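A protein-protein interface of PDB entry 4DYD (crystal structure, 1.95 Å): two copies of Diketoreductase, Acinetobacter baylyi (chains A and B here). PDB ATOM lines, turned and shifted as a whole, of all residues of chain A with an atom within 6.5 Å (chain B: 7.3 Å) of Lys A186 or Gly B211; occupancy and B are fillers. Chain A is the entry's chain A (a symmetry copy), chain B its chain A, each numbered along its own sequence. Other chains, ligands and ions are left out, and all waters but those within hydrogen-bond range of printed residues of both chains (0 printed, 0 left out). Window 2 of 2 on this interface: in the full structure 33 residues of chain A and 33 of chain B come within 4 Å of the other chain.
The side-chain amino group (NZ) of Lys A186 lies close to the backbone carbonyl oxygen (O) of Asp B210 (3.5 Å). N of Lys A185 is in hydrogen-bond range of O of Ile B212 (2.7 Å).
OD2 of Asp B210 sits close to OE1 of Glu B206, 2.5 Å away. The backbone carbonyl oxygen (O) of Leu B207 lies within hydrogen-bond range of the backbone NH (N) of Ile B212, at 2.8 Å. N of Lys A188 is in hydrogen-bond range of SD of Met A157, at 3.3 Å.
Leu A184 touches Ile B212 (CA to O, 3.4 Å). Gly B211 touches Lys A185 (O to CB, 3.4 Å). Lys A186 touches Gly B211 (CG to O, 3.7 Å). Lys A186 touches Ile B212 (O to CG2, 3.8 Å). Ile B212 touches Glu A187 (CD1 to O, 3.8 Å). Lys A188 touches Glu B206. CD2 of Leu B207 touches CG of Lys A188, 3.97 Å away. CG2 of Ile B212 touches CB of Lys A188, 3.8 Å away.
Of chain B, only Asp B210 (3.4 Å), Gly B211 (3.7 Å) and Ile B212 (3.8 Å) come within 4 Å of Lys A186. Gly B211 touches two residues of chain A. Printed residues of chain A within 4 Å of Ile B212: Leu A184 (3.4 Å), Lys A185 (2.7 Å), Lys A186 (3.8 Å), Glu A187 (3.8 Å) and Lys A188 (3.8 Å). Of the printed residues of chain B, Lys A185 touches Gly B211 (3.4 Å) and Ile B212 (2.7 Å). Of the printed residues of chain A, Leu B207 touches Lys A188. Ala B205 touches none of the printed residues of chain A. The nearest residue of chain B that does not touch Lys A186 is Ala B213 (5.9 Å).
Hydrophobic or aromatic side chains of chain B that line the printed part of chain A: Leu B207 and Ile B212. Hydrophobic or aromatic side chains of chain A that line the printed part of chain B: Leu A184. Among the printed residues, 10 pairs touch across the chains. Among the printed residues, no Asp or Glu carboxylate lies within 4 Å of a Lys or Arg side-chain nitrogen of the other chain.
No position is printed for both chains. Of the 10 pairs that touch across the chains among the printed residues, none has its exchanged pair printed and touching as well.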
ATOM      1  N   MET A 157      17.795  -1.219  -1.190  1.00  0.00           N
ATOM      2  CA  MET A 157      17.997  -2.446  -0.434  1.00  0.00           C
ATOM      3  C   MET A 157      18.035  -2.135   1.061  1.00  0.00           C
ATOM      4  O   MET A 157      18.942  -1.449   1.540  1.00  0.00           O
ATOM      5  CB  MET A 157      19.306  -3.102  -0.882  1.00  0.00           C
ATOM      6  CG  MET A 157      19.577  -4.480  -0.309  1.00  0.00           C
ATOM      7  SD  MET A 157      21.141  -5.161  -0.904  1.00  0.00           S
ATOM      8  CE  MET A 157      22.298  -4.087  -0.063  1.00  0.00           C
ATOM      9  N   GLY A 158      17.041  -2.628   1.794  1.00  0.00           N
ATOM     10  CA  GLY A 158      16.999  -2.389   3.226  1.00  0.00           C
ATOM     11  C   GLY A 158      17.419  -3.585   4.059  1.00  0.00           C
ATOM     12  O   GLY A 158      17.921  -4.578   3.526  1.00  0.00           O
ATOM     13  N   LEU A 184      15.337  -4.313  -4.428  1.00  0.00           N
ATOM     14  CA  LEU A 184      15.683  -5.588  -3.811  1.00  0.00           C
ATOM     15  C   LEU A 184      14.771  -5.883  -2.624  1.00  0.00           C
ATOM     16  O   LEU A 184      14.344  -4.973  -1.909  1.00  0.00           O
ATOM     17  CB  LEU A 184      17.158  -5.650  -3.395  1.00  0.00           C
ATOM     18  CG  LEU A 184      18.184  -5.679  -4.533  1.00  0.00           C
ATOM     19  CD1 LEU A 184      18.183  -4.361  -5.290  1.00  0.00           C
ATOM     20  CD2 LEU A 184      19.568  -5.953  -3.968  1.00  0.00           C
ATOM     21  N   LYS A 185      14.474  -7.165  -2.432  1.00  0.00           N
ATOM     22  CA  LYS A 185      13.549  -7.609  -1.397  1.00  0.00           C
ATOM     23  C   LYS A 185      14.303  -8.094  -0.158  1.00  0.00           C
ATOM     24  O   LYS A 185      13.742  -8.160   0.938  1.00  0.00           O
ATOM     25  CB  LYS A 185      12.677  -8.738  -1.950  1.00  0.00           C
ATOM     26  CG  LYS A 185      11.881  -8.341  -3.190  1.00  0.00           C
ATOM     27  CD  LYS A 185      11.129  -9.530  -3.772  1.00  0.00           C
ATOM     28  CE  LYS A 185      10.332  -9.130  -5.001  1.00  0.00           C
ATOM     29  NZ  LYS A 185       9.595 -10.283  -5.588  1.00  0.00           N
ATOM     30  N   LYS A 186      15.571  -8.440  -0.342  1.00  0.00           N
ATOM     31  CA  LYS A 186      16.422  -8.917   0.744  1.00  0.00           C
ATOM     32  C   LYS A 186      17.844  -8.419   0.516  1.00  0.00           C
ATOM     33  O   LYS A 186      18.242  -8.179  -0.626  1.00  0.00           O
ATOM     34  CB  LYS A 186      16.436 -10.449   0.774  1.00  0.00           C
ATOM     35  CG  LYS A 186      15.075 -11.101   0.939  1.00  0.00           C
ATOM     36  CD  LYS A 186      15.199 -12.619   0.957  1.00  0.00           C
ATOM     37  CE  LYS A 186      13.843 -13.289   1.120  1.00  0.00           C
ATOM     38  NZ  LYS A 186      13.950 -14.776   1.152  1.00  0.00           N
ATOM     39  N   GLU A 187      18.616  -8.270   1.588  1.00  0.00           N
ATOM     40  CA  GLU A 187      20.005  -7.860   1.435  1.00  0.00           C
ATOM     41  C   GLU A 187      20.803  -8.866   0.624  1.00  0.00           C
ATOM     42  O   GLU A 187      20.626 -10.080   0.752  1.00  0.00           O
ATOM     43  CB  GLU A 187      20.702  -7.630   2.778  1.00  0.00           C
ATOM     44  CG  GLU A 187      20.181  -6.458   3.577  1.00  0.00           C
ATOM     45  CD  GLU A 187      21.148  -6.040   4.667  1.00  0.00           C
ATOM     46  OE1 GLU A 187      22.114  -6.789   4.925  1.00  0.00           O
ATOM     47  OE2 GLU A 187      20.950  -4.961   5.259  1.00  0.00           O
ATOM     48  N   LYS A 188      21.686  -8.337  -0.209  1.00  0.00           N
ATOM     49  CA  LYS A 188      22.558  -9.139  -1.044  1.00  0.00           C
ATOM     50  C   LYS A 188      23.813  -8.329  -1.323  1.00  0.00           C
ATOM     51  O   LYS A 188      23.742  -7.216  -1.852  1.00  0.00           O
ATOM     52  CB  LYS A 188      21.851  -9.488  -2.361  1.00  0.00           C
ATOM     53  CG  LYS A 188      22.718 -10.214  -3.395  1.00  0.00           C
ATOM     54  CD  LYS A 188      23.162 -11.589  -2.918  1.00  0.00           C
ATOM     55  CE  LYS A 188      24.020 -12.288  -3.966  1.00  0.00           C
ATOM     56  NZ  LYS A 188      25.274 -11.536  -4.244  1.00  0.00           N
ATOM     57  N   ALA B 205      19.803 -16.724 -11.542  1.00  0.00           N
ATOM     58  CA  ALA B 205      18.985 -17.758 -10.914  1.00  0.00           C
ATOM     59  C   ALA B 205      19.065 -17.655  -9.390  1.00  0.00           C
ATOM     60  O   ALA B 205      18.047 -17.736  -8.697  1.00  0.00           O
ATOM     61  CB  ALA B 205      19.433 -19.134 -11.377  1.00  0.00           C
ATOM     62  N   GLU B 206      20.281 -17.472  -8.880  1.00  0.00           N
ATOM     63  CA  GLU B 206      20.506 -17.319  -7.444  1.00  0.00           C
ATOM     64  C   GLU B 206      19.720 -16.137  -6.889  1.00  0.00           C
ATOM     65  O   GLU B 206      19.034 -16.266  -5.872  1.00  0.00           O
ATOM     66  CB  GLU B 206      22.005 -17.175  -7.140  1.00  0.00           C
ATOM     67  CG  GLU B 206      22.345 -16.950  -5.661  1.00  0.00           C
ATOM     68  CD  GLU B 206      21.963 -15.563  -5.163  1.00  0.00           C
ATOM     69  OE1 GLU B 206      21.685 -15.412  -3.956  1.00  0.00           O
ATOM     70  OE2 GLU B 206      21.948 -14.618  -5.976  1.00  0.00           O
ATOM     71  N   LEU B 207      19.814 -14.986  -7.550  1.00  0.00           N
ATOM     72  CA  LEU B 207      19.043 -13.816  -7.134  1.00  0.00           C
ATOM     73  C   LEU B 207      17.550 -14.131  -7.069  1.00  0.00           C
ATOM     74  O   LEU B 207      16.859 -13.700  -6.142  1.00  0.00           O
ATOM     75  CB  LEU B 207      19.282 -12.636  -8.084  1.00  0.00           C
ATOM     76  CG  LEU B 207      20.700 -12.065  -8.127  1.00  0.00           C
ATOM     77  CD1 LEU B 207      20.840 -11.044  -9.246  1.00  0.00           C
ATOM     78  CD2 LEU B 207      21.055 -11.453  -6.779  1.00  0.00           C
ATOM     79  N   LEU B 208      17.048 -14.869  -8.057  1.00  0.00           N
ATOM     80  CA  LEU B 208      15.632 -15.219  -8.088  1.00  0.00           C
ATOM     81  C   LEU B 208      15.280 -16.191  -6.961  1.00  0.00           C
ATOM     82  O   LEU B 208      14.388 -15.916  -6.156  1.00  0.00           O
ATOM     83  CB  LEU B 208      15.244 -15.835  -9.435  1.00  0.00           C
ATOM     84  CG  LEU B 208      13.771 -16.222  -9.600  1.00  0.00           C
ATOM     85  CD1 LEU B 208      12.878 -14.995  -9.457  1.00  0.00           C
ATOM     86  CD2 LEU B 208      13.541 -16.885 -10.949  1.00  0.00           C
ATOM     87  N   VAL B 209      15.982 -17.319  -6.902  1.00  0.00           N
ATOM     88  CA  VAL B 209      15.652 -18.374  -5.946  1.00  0.00           C
ATOM     89  C   VAL B 209      15.769 -17.918  -4.496  1.00  0.00           C
ATOM     90  O   VAL B 209      14.981 -18.341  -3.648  1.00  0.00           O
ATOM     91  CB  VAL B 209      16.489 -19.647  -6.178  1.00  0.00           C
ATOM     92  CG1 VAL B 209      16.225 -20.656  -5.078  1.00  0.00           C
ATOM     93  CG2 VAL B 209      16.123 -20.261  -7.515  1.00  0.00           C
ATOM     94  N   ASP B 210      16.736 -17.056  -4.205  1.00  0.00           N
ATOM     95  CA  ASP B 210      16.906 -16.555  -2.848  1.00  0.00           C
ATOM     96  C   ASP B 210      16.013 -15.353  -2.582  1.00  0.00           C
ATOM     97  O   ASP B 210      16.126 -14.706  -1.539  1.00  0.00           O
ATOM     98  CB  ASP B 210      18.370 -16.214  -2.572  1.00  0.00           C
ATOM     99  CG  ASP B 210      19.266 -17.433  -2.632  1.00  0.00           C
ATOM    100  OD1 ASP B 210      18.729 -18.560  -2.574  1.00  0.00           O
ATOM    101  OD2 ASP B 210      20.501 -17.272  -2.735  1.00  0.00           O
ATOM    102  N   GLY B 211      15.124 -15.061  -3.526  1.00  0.00           N
ATOM    103  CA  GLY B 211      14.163 -13.987  -3.339  1.00  0.00           C
ATOM    104  C   GLY B 211      14.742 -12.585  -3.241  1.00  0.00           C
ATOM    105  O   GLY B 211      14.148 -11.712  -2.600  1.00  0.00           O
ATOM    106  N   ILE B 212      15.887 -12.343  -3.874  1.00  0.00           N
ATOM    107  CA  ILE B 212      16.484 -11.009  -3.829  1.00  0.00           C
ATOM    108  C   ILE B 212      15.700 -10.040  -4.713  1.00  0.00           C
ATOM    109  O   ILE B 212      15.455  -8.893  -4.328  1.00  0.00           O
ATOM    110  CB  ILE B 212      17.949 -11.015  -4.301  1.00  0.00           C
ATOM    111  CG1 ILE B 212      18.765 -12.051  -3.522  1.00  0.00           C
ATOM    112  CG2 ILE B 212      18.546  -9.618  -4.149  1.00  0.00           C
ATOM    113  CD1 ILE B 212      18.774 -11.841  -2.015  1.00  0.00           C
ATOM    114  N   ALA B 213      15.312 -10.505  -5.901  1.00  0.00           N
ATOM    115  CA  ALA B 213      14.574  -9.677  -6.852  1.00  0.00           C
ATOM    116  C   ALA B 213      13.808 -10.537  -7.858  1.00  0.00           C
ATOM    117  O   ALA B 213      14.129 -11.712  -8.054  1.00  0.00           O
ATOM    118  CB  ALA B 213      15.534  -8.749  -7.582  1.00  0.00           C
ATOM    119  N   ASP B 214      12.804  -9.952  -8.506  1.00  0.00           N
ATOM    120  CA  ASP B 214      12.023 -10.681  -9.504  1.00  0.00           C
ATOM    121  C   ASP B 214      12.721 -10.652 -10.876  1.00  0.00           C
ATOM    122  O   ASP B 214      13.631  -9.848 -11.102  1.00  0.00           O
ATOM    123  CB  ASP B 214      10.602 -10.113  -9.584  1.00  0.00           C
ATOM    124  CG  ASP B 214      10.575  -8.666 -10.021  1.00  0.00           C
ATOM    125  OD1 ASP B 214       9.471  -8.090 -10.111  1.00  0.00           O
ATOM    126  OD2 ASP B 214      11.657  -8.106 -10.284  1.00  0.00           O
